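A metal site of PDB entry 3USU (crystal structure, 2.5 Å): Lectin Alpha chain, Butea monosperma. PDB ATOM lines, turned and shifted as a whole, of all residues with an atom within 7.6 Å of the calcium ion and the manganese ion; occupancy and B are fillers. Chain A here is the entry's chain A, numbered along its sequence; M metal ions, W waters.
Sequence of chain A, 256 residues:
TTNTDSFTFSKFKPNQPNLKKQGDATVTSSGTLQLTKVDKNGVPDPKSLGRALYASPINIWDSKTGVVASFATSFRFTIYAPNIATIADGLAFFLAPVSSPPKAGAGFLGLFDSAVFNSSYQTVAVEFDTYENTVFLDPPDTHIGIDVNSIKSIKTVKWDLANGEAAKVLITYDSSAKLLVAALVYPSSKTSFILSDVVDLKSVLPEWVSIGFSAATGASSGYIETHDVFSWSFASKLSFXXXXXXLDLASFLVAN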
ATOM      1  N   ASP A  89      -1.605   2.388 -26.086  1.00  0.00           N
ATOM      2  CA  ASP A  89      -0.823   1.400 -25.444  1.00  0.00           C
ATOM      3  C   ASP A  89       0.629   1.422 -25.919  1.00  0.00           C
ATOM      4  O   ASP A  89       1.478   1.092 -25.193  1.00  0.00           O
ATOM      5  CB  ASP A  89      -1.446   0.087 -25.692  1.00  0.00           C
ATOM      6  CG  ASP A  89      -2.385  -0.307 -24.623  1.00  0.00           C
ATOM      7  OD1 ASP A  89      -3.562  -0.419 -24.892  1.00  0.00           O
ATOM      8  OD2 ASP A  89      -1.957  -0.480 -23.516  1.00  0.00           O
ATOM      9  N   GLY A  90       0.888   1.836 -27.146  1.00  0.00           N
ATOM     10  CA  GLY A  90       2.257   1.915 -27.686  1.00  0.00           C
ATOM     11  C   GLY A  90       2.416   1.707 -29.185  1.00  0.00           C
ATOM     12  O   GLY A  90       1.441   1.713 -29.935  1.00  0.00           O
ATOM     13  N   ALA A 106      -4.951  -3.374 -28.057  1.00  0.00           N
ATOM     14  CA  ALA A 106      -4.592  -2.932 -26.706  1.00  0.00           C
ATOM     15  C   ALA A 106      -3.070  -3.086 -26.357  1.00  0.00           C
ATOM     16  O   ALA A 106      -2.211  -2.927 -27.224  1.00  0.00           O
ATOM     17  CB  ALA A 106      -5.528  -3.560 -25.650  1.00  0.00           C
ATOM     18  N   GLY A 107      -2.746  -3.357 -25.094  1.00  0.00           N
ATOM     19  CA  GLY A 107      -1.370  -3.764 -24.695  1.00  0.00           C
ATOM     20  C   GLY A 107      -0.657  -4.936 -25.393  1.00  0.00           C
ATOM     21  O   GLY A 107       0.550  -5.138 -25.168  1.00  0.00           O
ATOM     22  N   PHE A 108      -1.387  -5.738 -26.187  1.00  0.00           N
ATOM     23  CA  PHE A 108      -0.760  -6.759 -27.037  1.00  0.00           C
ATOM     24  C   PHE A 108      -0.055  -6.135 -28.205  1.00  0.00           C
ATOM     25  O   PHE A 108       0.779  -6.773 -28.836  1.00  0.00           O
ATOM     26  CB  PHE A 108      -1.794  -7.727 -27.592  1.00  0.00           C
ATOM     27  CG  PHE A 108      -2.488  -8.503 -26.554  1.00  0.00           C
ATOM     28  CD1 PHE A 108      -1.922  -9.641 -26.034  1.00  0.00           C
ATOM     29  CD2 PHE A 108      -3.702  -8.072 -26.065  1.00  0.00           C
ATOM     30  CE1 PHE A 108      -2.557 -10.339 -25.041  1.00  0.00           C
ATOM     31  CE2 PHE A 108      -4.353  -8.777 -25.089  1.00  0.00           C
ATOM     32  CZ  PHE A 108      -3.790  -9.921 -24.581  1.00  0.00           C
ATOM     33  N   LEU A 109      -0.426  -4.885 -28.497  1.00  0.00           N
ATOM     34  CA  LEU A 109       0.297  -4.024 -29.432  1.00  0.00           C
ATOM     35  C   LEU A 109       0.208  -4.506 -30.885  1.00  0.00           C
ATOM     36  O   LEU A 109       1.058  -4.130 -31.722  1.00  0.00           O
ATOM     37  CB  LEU A 109       1.760  -3.869 -28.996  1.00  0.00           C
ATOM     38  CG  LEU A 109       2.087  -3.177 -27.682  1.00  0.00           C
ATOM     39  CD1 LEU A 109       3.600  -3.171 -27.532  1.00  0.00           C
ATOM     40  CD2 LEU A 109       1.545  -1.755 -27.622  1.00  0.00           C
ATOM     41  N   GLU A 127       9.517  -2.824 -28.357  1.00  0.00           N
ATOM     42  CA  GLU A 127       8.312  -2.093 -28.046  1.00  0.00           C
ATOM     43  C   GLU A 127       8.704  -0.791 -27.410  1.00  0.00           C
ATOM     44  O   GLU A 127       9.748  -0.668 -26.782  1.00  0.00           O
ATOM     45  CB  GLU A 127       7.369  -2.899 -27.149  1.00  0.00           C
ATOM     46  CG  GLU A 127       7.900  -3.151 -25.728  1.00  0.00           C
ATOM     47  CD  GLU A 127       6.939  -4.013 -24.929  1.00  0.00           C
ATOM     48  OE1 GLU A 127       6.445  -5.022 -25.483  1.00  0.00           O
ATOM     49  OE2 GLU A 127       6.656  -3.639 -23.774  1.00  0.00           O
ATOM     50  N   PHE A 128       7.815   0.181 -27.613  1.00  0.00           N
ATOM     51  CA  PHE A 128       7.865   1.483 -27.031  1.00  0.00           C
ATOM     52  C   PHE A 128       6.509   1.607 -26.370  1.00  0.00           C
ATOM     53  O   PHE A 128       5.544   2.043 -27.007  1.00  0.00           O
ATOM     54  CB  PHE A 128       8.030   2.533 -28.117  1.00  0.00           C
ATOM     55  CG  PHE A 128       9.287   2.374 -28.923  1.00  0.00           C
ATOM     56  CD1 PHE A 128      10.422   3.121 -28.622  1.00  0.00           C
ATOM     57  CD2 PHE A 128       9.338   1.499 -30.020  1.00  0.00           C
ATOM     58  CE1 PHE A 128      11.593   2.974 -29.372  1.00  0.00           C
ATOM     59  CE2 PHE A 128      10.480   1.365 -30.778  1.00  0.00           C
ATOM     60  CZ  PHE A 128      11.616   2.103 -30.456  1.00  0.00           C
ATOM     61  N   ASP A 129       6.476   1.222 -25.083  1.00  0.00           N
ATOM     62  CA  ASP A 129       5.255   0.900 -24.369  1.00  0.00           C
ATOM     63  C   ASP A 129       4.812   1.871 -23.312  1.00  0.00           C
ATOM     64  O   ASP A 129       5.514   2.170 -22.315  1.00  0.00           O
ATOM     65  CB  ASP A 129       5.340  -0.537 -23.823  1.00  0.00           C
ATOM     66  CG  ASP A 129       4.124  -0.945 -23.010  1.00  0.00           C
ATOM     67  OD1 ASP A 129       4.263  -1.903 -22.288  1.00  0.00           O
ATOM     68  OD2 ASP A 129       3.051  -0.330 -23.070  1.00  0.00           O
ATOM     69  N   THR A 130       3.552   2.232 -23.442  1.00  0.00           N
ATOM     70  CA  THR A 130       3.058   3.487 -22.904  1.00  0.00           C
ATOM     71  C   THR A 130       1.979   3.338 -21.793  1.00  0.00           C
ATOM     72  O   THR A 130       1.426   4.336 -21.282  1.00  0.00           O
ATOM     73  CB  THR A 130       2.561   4.229 -24.134  1.00  0.00           C
ATOM     74  OG1 THR A 130       3.117   5.535 -24.165  1.00  0.00           O
ATOM     75  CG2 THR A 130       1.081   4.193 -24.245  1.00  0.00           C
ATOM     76  N   TYR A 131       1.697   2.080 -21.408  1.00  0.00           N
ATOM     77  CA  TYR A 131       0.657   1.760 -20.440  1.00  0.00           C
ATOM     78  C   TYR A 131       1.083   0.498 -19.726  1.00  0.00           C
ATOM     79  O   TYR A 131       1.471  -0.469 -20.365  1.00  0.00           O
ATOM     80  CB  TYR A 131      -0.706   1.589 -21.120  1.00  0.00           C
ATOM     81  CG  TYR A 131      -1.835   1.071 -20.225  1.00  0.00           C
ATOM     82  CD1 TYR A 131      -2.648   1.949 -19.476  1.00  0.00           C
ATOM     83  CD2 TYR A 131      -2.095  -0.318 -20.112  1.00  0.00           C
ATOM     84  CE1 TYR A 131      -3.657   1.475 -18.673  1.00  0.00           C
ATOM     85  CE2 TYR A 131      -3.113  -0.800 -19.303  1.00  0.00           C
ATOM     86  CZ  TYR A 131      -3.898   0.111 -18.594  1.00  0.00           C
ATOM     87  OH  TYR A 131      -4.884  -0.368 -17.794  1.00  0.00           O
ATOM     88  N   GLU A 132       1.037   0.520 -18.389  1.00  0.00           N
ATOM     89  CA  GLU A 132       1.477  -0.606 -17.593  1.00  0.00           C
ATOM     90  C   GLU A 132       0.429  -1.750 -17.449  1.00  0.00           C
ATOM     91  O   GLU A 132      -0.469  -1.689 -16.593  1.00  0.00           O
ATOM     92  CB  GLU A 132       1.887  -0.130 -16.199  1.00  0.00           C
ATOM     93  CG  GLU A 132       2.656  -1.191 -15.451  1.00  0.00           C
ATOM     94  CD  GLU A 132       2.706  -1.001 -13.947  1.00  0.00           C
ATOM     95  OE1 GLU A 132       1.893  -0.265 -13.362  1.00  0.00           O
ATOM     96  OE2 GLU A 132       3.632  -1.586 -13.339  1.00  0.00           O
ATOM     97  N   ASN A 133       0.579  -2.777 -18.283  1.00  0.00           N
ATOM     98  CA  ASN A 133      -0.053  -4.074 -18.076  1.00  0.00           C
ATOM     99  C   ASN A 133       0.743  -4.929 -17.074  1.00  0.00           C
ATOM    100  O   ASN A 133       1.865  -5.384 -17.341  1.00  0.00           O
ATOM    101  CB  ASN A 133      -0.167  -4.824 -19.397  1.00  0.00           C
ATOM    102  CG  ASN A 133      -0.819  -3.989 -20.489  1.00  0.00           C
ATOM    103  OD1 ASN A 133      -2.016  -4.162 -20.803  1.00  0.00           O
ATOM    104  ND2 ASN A 133      -0.047  -3.078 -21.072  1.00  0.00           N
ATOM    105  N   THR A 134       0.117  -5.171 -15.923  1.00  0.00           N
ATOM    106  CA  THR A 134       0.804  -5.811 -14.840  1.00  0.00           C
ATOM    107  C   THR A 134       0.764  -7.282 -15.032  1.00  0.00           C
ATOM    108  O   THR A 134       1.673  -7.983 -14.580  1.00  0.00           O
ATOM    109  CB  THR A 134       0.201  -5.429 -13.497  1.00  0.00           C
ATOM    110  OG1 THR A 134      -1.192  -5.717 -13.519  1.00  0.00           O
ATOM    111  CG2 THR A 134       0.413  -3.931 -13.264  1.00  0.00           C
ATOM    112  N   PHE A 136       1.301  -8.273 -17.908  1.00  0.00           N
ATOM    113  CA  PHE A 136       2.457  -8.472 -18.806  1.00  0.00           C
ATOM    114  C   PHE A 136       3.780  -8.138 -18.134  1.00  0.00           C
ATOM    115  O   PHE A 136       4.795  -8.065 -18.818  1.00  0.00           O
ATOM    116  CB  PHE A 136       2.373  -7.712 -20.147  1.00  0.00           C
ATOM    117  CG  PHE A 136       1.096  -7.920 -20.918  1.00  0.00           C
ATOM    118  CD1 PHE A 136       0.347  -9.110 -20.793  1.00  0.00           C
ATOM    119  CD2 PHE A 136       0.616  -6.925 -21.785  1.00  0.00           C
ATOM    120  CE1 PHE A 136      -0.861  -9.291 -21.505  1.00  0.00           C
ATOM    121  CE2 PHE A 136      -0.585  -7.108 -22.474  1.00  0.00           C
ATOM    122  CZ  PHE A 136      -1.317  -8.291 -22.332  1.00  0.00           C
ATOM    123  N   LEU A 137       3.794  -7.984 -16.805  1.00  0.00           N
ATOM    124  CA  LEU A 137       5.034  -7.718 -16.062  1.00  0.00           C
ATOM    125  C   LEU A 137       5.665  -6.363 -16.444  1.00  0.00           C
ATOM    126  O   LEU A 137       6.867  -6.159 -16.316  1.00  0.00           O
ATOM    127  CB  LEU A 137       6.032  -8.881 -16.203  1.00  0.00           C
ATOM    128  CG  LEU A 137       5.606 -10.327 -15.866  1.00  0.00           C
ATOM    129  CD1 LEU A 137       6.842 -11.163 -15.614  1.00  0.00           C
ATOM    130  CD2 LEU A 137       4.627 -10.462 -14.698  1.00  0.00           C
ATOM    131  N   ASP A 138       4.813  -5.466 -16.918  1.00  0.00           N
ATOM    132  CA  ASP A 138       5.168  -4.136 -17.260  1.00  0.00           C
ATOM    133  C   ASP A 138       5.639  -3.370 -16.059  1.00  0.00           C
ATOM    134  O   ASP A 138       5.035  -3.477 -14.981  1.00  0.00           O
ATOM    135  CB  ASP A 138       3.960  -3.382 -17.777  1.00  0.00           C
ATOM    136  CG  ASP A 138       3.899  -3.362 -19.263  1.00  0.00           C
ATOM    137  OD1 ASP A 138       4.931  -3.597 -19.910  1.00  0.00           O
ATOM    138  OD2 ASP A 138       2.811  -3.103 -19.812  1.00  0.00           O
ATOM    139  N   PRO A 139       6.678  -2.565 -16.242  1.00  0.00           N
ATOM    140  CA  PRO A 139       7.131  -1.671 -15.214  1.00  0.00           C
ATOM    141  C   PRO A 139       6.202  -0.446 -15.170  1.00  0.00           C
ATOM    142  O   PRO A 139       5.564  -0.100 -16.182  1.00  0.00           O
ATOM    143  CB  PRO A 139       8.553  -1.334 -15.645  1.00  0.00           C
ATOM    144  CG  PRO A 139       8.570  -1.466 -17.130  1.00  0.00           C
ATOM    145  CD  PRO A 139       7.468  -2.455 -17.488  1.00  0.00           C
ATOM    146  N   ASP A 141       6.614   2.673 -15.216  1.00  0.00           N
ATOM    147  CA  ASP A 141       6.960   3.772 -16.096  1.00  0.00           C
ATOM    148  C   ASP A 141       6.884   3.348 -17.549  1.00  0.00           C
ATOM    149  O   ASP A 141       7.011   2.180 -17.853  1.00  0.00           O
ATOM    150  CB  ASP A 141       8.391   4.185 -15.781  1.00  0.00           C
ATOM    151  CG  ASP A 141       9.370   3.006 -15.910  1.00  0.00           C
ATOM    152  OD1 ASP A 141       9.950   2.887 -17.030  1.00  0.00           O
ATOM    153  OD2 ASP A 141       9.503   2.189 -14.941  1.00  0.00           O
ATOM    154  N   HIS A 143       8.360   2.832 -21.114  1.00  0.00           N
ATOM    155  CA  HIS A 143       9.601   2.051 -21.248  1.00  0.00           C
ATOM    156  C   HIS A 143       9.776   1.551 -22.644  1.00  0.00           C
ATOM    157  O   HIS A 143       8.817   1.509 -23.415  1.00  0.00           O
ATOM    158  CB  HIS A 143       9.630   0.861 -20.301  1.00  0.00           C
ATOM    159  CG  HIS A 143       8.481  -0.108 -20.503  1.00  0.00           C
ATOM    160  ND1 HIS A 143       7.218   0.240 -20.317  1.00  0.00           N
ATOM    161  CD2 HIS A 143       8.466  -1.441 -20.885  1.00  0.00           C
ATOM    162  CE1 HIS A 143       6.427  -0.821 -20.554  1.00  0.00           C
ATOM    163  NE2 HIS A 143       7.186  -1.835 -20.922  1.00  0.00           N
ATOM    164  N   ILE A 144      11.016   1.252 -23.003  1.00  0.00           N
ATOM    165  CA  ILE A 144      11.326   0.628 -24.281  1.00  0.00           C
ATOM    166  C   ILE A 144      11.594  -0.820 -23.897  1.00  0.00           C
ATOM    167  O   ILE A 144      12.300  -1.059 -22.914  1.00  0.00           O
ATOM    168  CB  ILE A 144      12.577   1.255 -24.888  1.00  0.00           C
ATOM    169  CG1 ILE A 144      12.250   2.599 -25.506  1.00  0.00           C
ATOM    170  CG2 ILE A 144      13.180   0.358 -25.957  1.00  0.00           C
ATOM    171  CD1 ILE A 144      13.408   3.583 -25.459  1.00  0.00           C
ATOM    172  N   GLY A 145      11.012  -1.761 -24.634  1.00  0.00           N
ATOM    173  CA  GLY A 145      11.182  -3.182 -24.376  1.00  0.00           C
ATOM    174  C   GLY A 145      11.836  -3.866 -25.563  1.00  0.00           C
ATOM    175  O   GLY A 145      11.701  -3.378 -26.674  1.00  0.00           O
ATOM    176  N   ASP A 147      11.268  -7.609 -27.094  1.00  0.00           N
ATOM    177  CA  ASP A 147      10.303  -8.735 -26.930  1.00  0.00           C
ATOM    178  C   ASP A 147      10.594  -9.857 -27.906  1.00  0.00           C
ATOM    179  O   ASP A 147      10.693  -9.612 -29.090  1.00  0.00           O
ATOM    180  CB  ASP A 147       8.868  -8.296 -27.251  1.00  0.00           C
ATOM    181  CG  ASP A 147       8.348  -7.200 -26.367  1.00  0.00           C
ATOM    182  OD1 ASP A 147       8.832  -6.994 -25.253  1.00  0.00           O
ATOM    183  OD2 ASP A 147       7.396  -6.510 -26.802  1.00  0.00           O
ATOM    184  N   ILE A 151       4.802 -10.835 -24.916  1.00  0.00           N
ATOM    185  CA  ILE A 151       4.601  -9.417 -24.589  1.00  0.00           C
ATOM    186  C   ILE A 151       5.393  -8.973 -23.322  1.00  0.00           C
ATOM    187  O   ILE A 151       5.639  -7.773 -23.078  1.00  0.00           O
ATOM    188  CB  ILE A 151       3.094  -9.078 -24.541  1.00  0.00           C
ATOM    189  CG1 ILE A 151       2.837  -7.571 -24.618  1.00  0.00           C
ATOM    190  CG2 ILE A 151       2.437  -9.663 -23.299  1.00  0.00           C
ATOM    191  CD1 ILE A 151       3.222  -6.902 -25.923  1.00  0.00           C
ATOM    192  N   LYS A 152       5.773  -9.988 -22.534  1.00  0.00           N
ATOM    193  CA  LYS A 152       6.593  -9.818 -21.372  1.00  0.00           C
ATOM    194  C   LYS A 152       7.956  -9.693 -21.941  1.00  0.00           C
ATOM    195  O   LYS A 152       8.624 -10.686 -22.200  1.00  0.00           O
ATOM    196  CB  LYS A 152       6.504 -11.034 -20.448  1.00  0.00           C
ATOM    197  CG  LYS A 152       5.081 -11.483 -20.115  1.00  0.00           C
ATOM    198  CD  LYS A 152       5.124 -12.742 -19.267  1.00  0.00           C
ATOM    199  CE  LYS A 152       4.195 -12.628 -18.066  1.00  0.00           C
ATOM    200  NZ  LYS A 152       3.497 -13.925 -17.818  1.00  0.00           N
ATOM    201  N   SER A 153       8.353  -8.437 -22.159  1.00  0.00           N
ATOM    202  CA  SER A 153       9.697  -8.067 -22.539  1.00  0.00           C
ATOM    203  C   SER A 153      10.730  -8.827 -21.732  1.00  0.00           C
ATOM    204  O   SER A 153      10.542  -9.077 -20.548  1.00  0.00           O
ATOM    205  CB  SER A 153       9.893  -6.584 -22.302  1.00  0.00           C
ATOM    206  OG  SER A 153       8.843  -5.820 -22.912  1.00  0.00           O
ATOM    207  N   THR A 156      13.756  -4.445 -20.359  1.00  0.00           N
ATOM    208  CA  THR A 156      13.202  -3.134 -20.581  1.00  0.00           C
ATOM    209  C   THR A 156      14.158  -2.039 -20.070  1.00  0.00           C
ATOM    210  O   THR A 156      15.141  -2.320 -19.410  1.00  0.00           O
ATOM    211  CB  THR A 156      11.822  -3.005 -19.916  1.00  0.00           C
ATOM    212  OG1 THR A 156      12.010  -2.856 -18.506  1.00  0.00           O
ATOM    213  CG2 THR A 156      10.937  -4.231 -20.192  1.00  0.00           C
HETATM  214 CA    CA M   1       1.902  -2.342 -21.841  1.00  0.00          CA
HETATM  215 MN    MN M   2       5.855  -3.502 -21.952  1.00  0.00          MN
HETATM  216  O   HOH W   1       2.525  -3.971 -22.895  1.00  0.00           O
HETATM  217  O   HOH W   2       4.641  -5.468 -22.910  1.00  0.00           O
HETATM  218  O   HOH W   3       0.739  -1.476 -23.447  1.00  0.00           O
HETATM  219  O   HOH W   4       7.506  -4.874 -21.242  1.00  0.00           O
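Four residues have an atom within 4 Å of the calcium ion: Asp 129, Tyr 131, Asn 133 and Asp 138.
The nearest printed residue that does not touch the calcium ion is Gly 107 (4.6 Å).
The manganese ion is bound by OE2 of Glu 127 (2.0 Å), OD1 of Asp 138 (2.2 Å), water W4 (2.3 Å), OD1 of Asp 129 (2.3 Å), NE2 of His 143 (2.4 Å) and water W2 (2.5 Å).
The manganese ion has six donor atoms within binding distance.
OE2 of Glu 127 sits close to OG of Ser 153 (3.2 Å).
The backbone carbonyl oxygen (O) of Glu 127 sits at hydrogen-bond distance from the backbone NH (N) of Gly 145, at 2.7 Å.
O of Asp 141 is in hydrogen-bond range of ND1 of His 143 (3.1 Å).
OG of Ser 153 lies within hydrogen-bond range of OD1 of Asp 147.
Water W2 bridges the backbone carbonyl oxygen of Ile 151 (2.5 Å) and the side-chain carboxylate of Glu 127 (3.2 Å).
OG of Ser 153 touches the manganese ion (3.9 Å).
Of the 27 residues printed, 5 come within 4 Å of the manganese ion.
The calcium ion is bound by water W1 (2.0 Å).
Water W3 is bound to the calcium ion, at 2.2 Å.
ND2 of Asn 133 is bound to the calcium ion (2.2 Å).
OD2 of Asp 138 binds the calcium ion, at 2.3 Å.
The calcium ion is bound by the backbone carbonyl oxygen (O) of Tyr 131 (2.4 Å).
The calcium ion is bound by OD1 of Asp 129 (2.4 Å).
OD2 of Asp 129 is bound to the calcium ion, at 2.6 Å.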
